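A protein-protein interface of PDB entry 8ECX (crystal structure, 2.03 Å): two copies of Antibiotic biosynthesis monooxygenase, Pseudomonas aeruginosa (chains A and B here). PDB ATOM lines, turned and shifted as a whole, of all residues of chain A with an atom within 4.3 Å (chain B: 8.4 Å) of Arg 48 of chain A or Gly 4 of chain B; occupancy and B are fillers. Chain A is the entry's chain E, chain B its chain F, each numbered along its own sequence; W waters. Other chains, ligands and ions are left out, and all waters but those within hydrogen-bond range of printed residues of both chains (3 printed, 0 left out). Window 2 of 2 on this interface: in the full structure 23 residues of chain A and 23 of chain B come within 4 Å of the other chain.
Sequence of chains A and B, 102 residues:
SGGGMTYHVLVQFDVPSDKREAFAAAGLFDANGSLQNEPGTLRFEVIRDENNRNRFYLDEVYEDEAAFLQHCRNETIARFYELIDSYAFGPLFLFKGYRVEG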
ATOM      1  N   ILE A  47      16.576  -2.567  -9.562  1.00  0.00           N
ATOM      2  CA  ILE A  47      16.544  -1.516 -10.569  1.00  0.00           C
ATOM      3  C   ILE A  47      15.124  -0.981 -10.677  1.00  0.00           C
ATOM      4  O   ILE A  47      14.161  -1.754 -10.715  1.00  0.00           O
ATOM      5  CB  ILE A  47      17.039  -2.033 -11.937  1.00  0.00           C
ATOM      6  CG1 ILE A  47      18.451  -2.610 -11.814  1.00  0.00           C
ATOM      7  CG2 ILE A  47      17.015  -0.926 -12.978  1.00  0.00           C
ATOM      8  CD1 ILE A  47      18.871  -3.435 -13.002  1.00  0.00           C
ATOM      9  N   ARG A  48      14.997   0.341 -10.722  1.00  0.00           N
ATOM     10  CA  ARG A  48      13.721   0.999 -10.959  1.00  0.00           C
ATOM     11  C   ARG A  48      13.664   1.477 -12.404  1.00  0.00           C
ATOM     12  O   ARG A  48      14.669   1.936 -12.955  1.00  0.00           O
ATOM     13  CB  ARG A  48      13.520   2.180 -10.006  1.00  0.00           C
ATOM     14  CG  ARG A  48      14.513   3.314 -10.196  1.00  0.00           C
ATOM     15  CD  ARG A  48      14.302   4.421  -9.183  1.00  0.00           C
ATOM     16  NE  ARG A  48      15.251   5.511  -9.380  1.00  0.00           N
ATOM     17  CZ  ARG A  48      15.058   6.531 -10.206  1.00  0.00           C
ATOM     18  NH1 ARG A  48      13.945   6.649 -10.911  1.00  0.00           N
ATOM     19  NH2 ARG A  48      16.006   7.457 -10.326  1.00  0.00           N
ATOM     20  N   ASP A  49      12.491   1.352 -13.020  1.00  0.00           N
ATOM     21  CA  ASP A  49      12.333   1.798 -14.398  1.00  0.00           C
ATOM     22  C   ASP A  49      12.512   3.309 -14.483  1.00  0.00           C
ATOM     23  O   ASP A  49      12.086   4.051 -13.595  1.00  0.00           O
ATOM     24  CB  ASP A  49      10.959   1.403 -14.939  1.00  0.00           C
ATOM     25  CG  ASP A  49      10.863   1.546 -16.444  1.00  0.00           C
ATOM     26  OD1 ASP A  49      11.241   0.594 -17.159  1.00  0.00           O
ATOM     27  OD2 ASP A  49      10.426   2.620 -16.911  1.00  0.00           O
ATOM     28  N   GLU A  50      13.153   3.761 -15.563  1.00  0.00           N
ATOM     29  CA  GLU A  50      13.469   5.181 -15.688  1.00  0.00           C
ATOM     30  C   GLU A  50      12.212   6.041 -15.786  1.00  0.00           C
ATOM     31  O   GLU A  50      12.243   7.223 -15.423  1.00  0.00           O
ATOM     32  CB  GLU A  50      14.379   5.417 -16.897  1.00  0.00           C
ATOM     33  CG  GLU A  50      13.692   5.344 -18.255  1.00  0.00           C
ATOM     34  CD  GLU A  50      14.642   5.662 -19.399  1.00  0.00           C
ATOM     35  OE1 GLU A  50      15.755   6.164 -19.128  1.00  0.00           O
ATOM     36  OE2 GLU A  50      14.283   5.412 -20.567  1.00  0.00           O
ATOM     37  N   ARG A  55       7.162   0.111 -11.638  1.00  0.00           N
ATOM     38  CA  ARG A  55       7.812  -1.075 -12.179  1.00  0.00           C
ATOM     39  C   ARG A  55       9.247  -1.174 -11.676  1.00  0.00           C
ATOM     40  O   ARG A  55      10.000  -0.195 -11.727  1.00  0.00           O
ATOM     41  CB  ARG A  55       7.789  -1.055 -13.709  1.00  0.00           C
ATOM     42  CG  ARG A  55       8.466  -2.254 -14.341  1.00  0.00           C
ATOM     43  CD  ARG A  55       7.936  -2.513 -15.737  1.00  0.00           C
ATOM     44  NE  ARG A  55       6.579  -3.046 -15.724  1.00  0.00           N
ATOM     45  CZ  ARG A  55       5.905  -3.399 -16.809  1.00  0.00           C
ATOM     46  NH1 ARG A  55       6.428  -3.277 -18.018  1.00  0.00           N
ATOM     47  NH2 ARG A  55       4.675  -3.888 -16.678  1.00  0.00           N
ATOM     48  N   PHE A  56       9.621  -2.363 -11.211  1.00  0.00           N
ATOM     49  CA  PHE A  56      10.967  -2.632 -10.731  1.00  0.00           C
ATOM     50  C   PHE A  56      11.505  -3.896 -11.385  1.00  0.00           C
ATOM     51  O   PHE A  56      10.750  -4.740 -11.875  1.00  0.00           O
ATOM     52  CB  PHE A  56      11.011  -2.794  -9.206  1.00  0.00           C
ATOM     53  CG  PHE A  56      10.650  -1.550  -8.456  1.00  0.00           C
ATOM     54  CD1 PHE A  56      11.638  -0.742  -7.918  1.00  0.00           C
ATOM     55  CD2 PHE A  56       9.324  -1.195  -8.276  1.00  0.00           C
ATOM     56  CE1 PHE A  56      11.310   0.409  -7.224  1.00  0.00           C
ATOM     57  CE2 PHE A  56       8.986  -0.046  -7.584  1.00  0.00           C
ATOM     58  CZ  PHE A  56       9.981   0.755  -7.053  1.00  0.00           C
ATOM     59  N   GLY B   4      18.635   7.393  -8.709  1.00  0.00           N
ATOM     60  CA  GLY B   4      19.562   6.566  -7.961  1.00  0.00           C
ATOM     61  C   GLY B   4      20.959   6.558  -8.551  1.00  0.00           C
ATOM     62  O   GLY B   4      21.421   7.556  -9.098  1.00  0.00           O
ATOM     63  N   MET B   5      21.632   5.414  -8.443  1.00  0.00           N
ATOM     64  CA  MET B   5      23.005   5.286  -8.916  1.00  0.00           C
ATOM     65  C   MET B   5      23.090   5.092 -10.426  1.00  0.00           C
ATOM     66  O   MET B   5      22.655   5.941 -11.209  1.00  0.00           O
ATOM     67  CB  MET B   5      23.699   4.113  -8.214  1.00  0.00           C
ATOM     68  CG  MET B   5      24.440   4.472  -6.936  1.00  0.00           C
ATOM     69  SD  MET B   5      26.217   4.650  -7.200  1.00  0.00           S
ATOM     70  CE  MET B   5      26.783   2.977  -6.907  1.00  0.00           C
ATOM     71  N   THR B   6      23.645   3.954 -10.818  1.00  0.00           N
ATOM     72  CA  THR B   6      24.015   3.616 -12.188  1.00  0.00           C
ATOM     73  C   THR B   6      22.799   3.390 -13.086  1.00  0.00           C
ATOM     74  O   THR B   6      21.691   3.086 -12.633  1.00  0.00           O
ATOM     75  CB  THR B   6      24.912   2.377 -12.206  1.00  0.00           C
ATOM     76  OG1 THR B   6      24.282   1.313 -11.481  1.00  0.00           O
ATOM     77  CG2 THR B   6      26.259   2.697 -11.572  1.00  0.00           C
ATOM     78  N   TYR B   7      23.041   3.534 -14.387  1.00  0.00           N
ATOM     79  CA  TYR B   7      22.019   3.506 -15.428  1.00  0.00           C
ATOM     80  C   TYR B   7      22.118   2.183 -16.176  1.00  0.00           C
ATOM     81  O   TYR B   7      23.139   1.902 -16.814  1.00  0.00           O
ATOM     82  CB  TYR B   7      22.204   4.688 -16.380  1.00  0.00           C
ATOM     83  CG  TYR B   7      21.111   4.868 -17.409  1.00  0.00           C
ATOM     84  CD1 TYR B   7      19.822   5.208 -17.027  1.00  0.00           C
ATOM     85  CD2 TYR B   7      21.377   4.723 -18.764  1.00  0.00           C
ATOM     86  CE1 TYR B   7      18.821   5.384 -17.965  1.00  0.00           C
ATOM     87  CE2 TYR B   7      20.384   4.897 -19.709  1.00  0.00           C
ATOM     88  CZ  TYR B   7      19.106   5.227 -19.306  1.00  0.00           C
ATOM     89  OH  TYR B   7      18.113   5.399 -20.248  1.00  0.00           O
ATOM     90  N   HIS B   8      21.061   1.378 -16.103  1.00  0.00           N
ATOM     91  CA  HIS B   8      21.073   0.012 -16.608  1.00  0.00           C
ATOM     92  C   HIS B   8      20.223  -0.084 -17.866  1.00  0.00           C
ATOM     93  O   HIS B   8      19.102   0.431 -17.904  1.00  0.00           O
ATOM     94  CB  HIS B   8      20.564  -0.962 -15.545  1.00  0.00           C
ATOM     95  CG  HIS B   8      21.459  -1.067 -14.351  1.00  0.00           C
ATOM     96  ND1 HIS B   8      21.877  -2.274 -13.835  1.00  0.00           N
ATOM     97  CD2 HIS B   8      22.030  -0.111 -13.578  1.00  0.00           C
ATOM     98  CE1 HIS B   8      22.660  -2.060 -12.795  1.00  0.00           C
ATOM     99  NE2 HIS B   8      22.767  -0.756 -12.616  1.00  0.00           N
ATOM    100  N   GLU B  63      27.492   4.998 -16.263  1.00  0.00           N
ATOM    101  CA  GLU B  63      27.559   5.927 -15.141  1.00  0.00           C
ATOM    102  C   GLU B  63      26.273   6.731 -15.006  1.00  0.00           C
ATOM    103  O   GLU B  63      25.838   7.020 -13.885  1.00  0.00           O
ATOM    104  CB  GLU B  63      28.759   6.860 -15.300  1.00  0.00           C
ATOM    105  N   ASP B  64      25.650   7.082 -16.125  1.00  0.00           N
ATOM    106  CA  ASP B  64      24.380   7.800 -16.142  1.00  0.00           C
ATOM    107  C   ASP B  64      23.808   7.703 -17.553  1.00  0.00           C
ATOM    108  O   ASP B  64      24.375   7.041 -18.428  1.00  0.00           O
ATOM    109  CB  ASP B  64      24.550   9.252 -15.682  1.00  0.00           C
ATOM    110  CG  ASP B  64      25.601  10.005 -16.482  1.00  0.00           C
ATOM    111  OD1 ASP B  64      26.060   9.490 -17.524  1.00  0.00           O
ATOM    112  OD2 ASP B  64      25.974  11.120 -16.060  1.00  0.00           O
ATOM    113  N   PHE B  95      14.289  -2.896 -20.905  1.00  0.00           N
ATOM    114  CA  PHE B  95      14.068  -1.756 -20.026  1.00  0.00           C
ATOM    115  C   PHE B  95      15.309  -0.877 -20.007  1.00  0.00           C
ATOM    116  O   PHE B  95      16.398  -1.286 -20.423  1.00  0.00           O
ATOM    117  CB  PHE B  95      13.691  -2.188 -18.598  1.00  0.00           C
ATOM    118  CG  PHE B  95      14.804  -2.863 -17.827  1.00  0.00           C
ATOM    119  CD1 PHE B  95      15.859  -2.133 -17.289  1.00  0.00           C
ATOM    120  CD2 PHE B  95      14.770  -4.231 -17.608  1.00  0.00           C
ATOM    121  CE1 PHE B  95      16.867  -2.756 -16.576  1.00  0.00           C
ATOM    122  CE2 PHE B  95      15.773  -4.860 -16.894  1.00  0.00           C
ATOM    123  CZ  PHE B  95      16.824  -4.122 -16.378  1.00  0.00           C
ATOM    124  N   LYS B  96      15.114   0.342 -19.516  1.00  0.00           N
ATOM    125  CA  LYS B  96      16.179   1.235 -19.091  1.00  0.00           C
ATOM    126  C   LYS B  96      15.802   1.765 -17.715  1.00  0.00           C
ATOM    127  O   LYS B  96      14.635   2.078 -17.464  1.00  0.00           O
ATOM    128  CB  LYS B  96      16.382   2.384 -20.088  1.00  0.00           C
ATOM    129  CG  LYS B  96      16.878   1.928 -21.453  1.00  0.00           C
ATOM    130  CD  LYS B  96      17.099   3.096 -22.392  1.00  0.00           C
ATOM    131  CE  LYS B  96      15.784   3.548 -23.002  1.00  0.00           C
ATOM    132  NZ  LYS B  96      15.569   2.964 -24.353  1.00  0.00           N
ATOM    133  N   GLY B  97      16.776   1.829 -16.815  1.00  0.00           N
ATOM    134  CA  GLY B  97      16.441   2.222 -15.459  1.00  0.00           C
ATOM    135  C   GLY B  97      17.671   2.548 -14.644  1.00  0.00           C
ATOM    136  O   GLY B  97      18.801   2.536 -15.138  1.00  0.00           O
ATOM    137  N   TYR B  98      17.424   2.840 -13.369  1.00  0.00           N
ATOM    138  CA  TYR B  98      18.456   3.249 -12.429  1.00  0.00           C
ATOM    139  C   TYR B  98      18.523   2.263 -11.275  1.00  0.00           C
ATOM    140  O   TYR B  98      17.490   1.800 -10.779  1.00  0.00           O
ATOM    141  CB  TYR B  98      18.183   4.658 -11.899  1.00  0.00           C
ATOM    142  CG  TYR B  98      18.315   5.724 -12.955  1.00  0.00           C
ATOM    143  CD1 TYR B  98      19.537   6.333 -13.206  1.00  0.00           C
ATOM    144  CD2 TYR B  98      17.219   6.113 -13.712  1.00  0.00           C
ATOM    145  CE1 TYR B  98      19.662   7.304 -14.179  1.00  0.00           C
ATOM    146  CE2 TYR B  98      17.334   7.083 -14.687  1.00  0.00           C
ATOM    147  CZ  TYR B  98      18.557   7.676 -14.916  1.00  0.00           C
ATOM    148  OH  TYR B  98      18.676   8.645 -15.885  1.00  0.00           O
ATOM    149  N   ARG B  99      19.742   1.944 -10.850  1.00  0.00           N
ATOM    150  CA  ARG B  99      19.923   1.038  -9.728  1.00  0.00           C
ATOM    151  C   ARG B  99      19.439   1.683  -8.437  1.00  0.00           C
ATOM    152  O   ARG B  99      19.697   2.860  -8.176  1.00  0.00           O
ATOM    153  CB  ARG B  99      21.392   0.642  -9.589  1.00  0.00           C
ATOM    154  CG  ARG B  99      21.631  -0.408  -8.519  1.00  0.00           C
ATOM    155  CD  ARG B  99      23.099  -0.744  -8.357  1.00  0.00           C
ATOM    156  NE  ARG B  99      23.284  -1.829  -7.399  1.00  0.00           N
ATOM    157  CZ  ARG B  99      24.461  -2.309  -7.023  1.00  0.00           C
ATOM    158  NH1 ARG B  99      25.593  -1.826  -7.511  1.00  0.00           N
ATOM    159  NH2 ARG B  99      24.505  -3.300  -6.138  1.00  0.00           N
ATOM    160  N   VAL B 100      18.730   0.903  -7.628  1.00  0.00           N
ATOM    161  CA  VAL B 100      18.274   1.369  -6.323  1.00  0.00           C
ATOM    162  C   VAL B 100      19.410   1.179  -5.324  1.00  0.00           C
ATOM    163  O   VAL B 100      19.925   0.069  -5.155  1.00  0.00           O
ATOM    164  CB  VAL B 100      17.008   0.622  -5.881  1.00  0.00           C
ATOM    165  CG1 VAL B 100      16.641   0.994  -4.455  1.00  0.00           C
ATOM    166  CG2 VAL B 100      15.858   0.926  -6.831  1.00  0.00           C
ATOM    167  N   GLU B 101      19.806   2.266  -4.666  1.00  0.00           N
ATOM    168  CA  GLU B 101      20.977   2.250  -3.801  1.00  0.00           C
ATOM    169  C   GLU B 101      20.647   1.659  -2.437  1.00  0.00           C
ATOM    170  O   GLU B 101      19.589   1.932  -1.862  1.00  0.00           O
ATOM    171  CB  GLU B 101      21.533   3.663  -3.632  1.00  0.00           C
HETATM  172  O   HOH W   1      12.275   1.051 -19.667  1.00  0.00           O
HETATM  173  O   HOH W   2      17.367   3.990  -8.328  1.00  0.00           O
HETATM  174  O   HOH W   3      16.544   8.357 -17.814  1.00  0.00           O
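The backbone NH (N) of Arg 48 of chain A is in hydrogen-bond range of the backbone carbonyl oxygen (O) of Tyr 98 of chain B, 2.9 Å away. The side-chain carboxylate of Glu 50 of chain A lies within hydrogen-bond range of the side-chain hydroxyl of Tyr 7 of chain B (2.7 Å). The backbone NH of Glu 50 of chain A is in hydrogen-bond range of the backbone carbonyl oxygen of Lys 96 of chain B, 2.9 Å away. NH2 of Arg 48 of chain A lies close to N of Gly 4 of chain B, 3.1 Å away.
The backbone NH (N) of Asp 49 of chain A lies within hydrogen-bond range of the backbone carbonyl oxygen (O) of Arg 55 of chain A (3.2 Å). A ring nitrogen (NE2) of His 8 of chain B lies within hydrogen-bond range of the side-chain hydroxyl (OG1) of Thr 6 of chain B (2.8 Å). O of Gly 97 of chain B is in hydrogen-bond range of N of His 8 of chain B (2.7 Å).
CD1 of Ile 47 of chain A touches ND1 of His 8 of chain B, at 3.3 Å. Ile 47 of chain A touches Gly 97 of chain B (CG2 to C, 3.9 Å). Ile 47 of chain A touches Tyr 98 of chain B. Arg 48 of chain A touches Gly 97 of chain B (O to CA, 3.1 Å). OD1 of Asp 49 of chain A touches CB of Phe 95 of chain B, at 3.98 Å. O of Lys 96 of chain B touches OD1 of Asp 49 of chain A, at 3.7 Å. Gly 97 of chain B touches Glu 50 of chain A.
Printed residues of chain A within 4 Å of Gly 4 of chain B: Arg 48. Of the printed residues of chain B, Glu 50 of chain A touches Tyr 7, Lys 96 and Gly 97. Of the printed residues of chain B, Asp 49 of chain A touches Phe 95 and Lys 96. Glu 63 of chain B touches none of the printed residues of chain A. The nearest printed residue of chain A that does not touch Phe 95 of chain B is Ile 47 of chain A (4.01 Å).
Of the 14 printed residues of chain B, 7 touch a printed residue of chain A. Of the 6 printed residues of chain A, 4 touch a printed residue of chain B. Among the printed residues, 11 pairs touch across the chains.
No position is printed for both chains. Of the 11 pairs that touch across the chains among the printed residues, none has its exchanged pair printed and touching as well.
Water W2 lies within hydrogen-bond range of the backbone carbonyl oxygen of Arg 99 of chain B, the guanidinium group of Arg 48 of chain A, the backbone carbonyl oxygen of Tyr 98 of chain B and the backbone NH of Val 100 of chain B. Water W3 lies within hydrogen-bond range of the side-chain carboxylate (OE1) of Glu 50 of chain A (2.7 Å) and the side-chain hydroxyl (OH) of Tyr 98 of chain B (2.9 Å). Water W1 bridges OD1 of Asp 49 of chain A (2.8 Å) and N of Lys 96 of chain B (2.9 Å).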
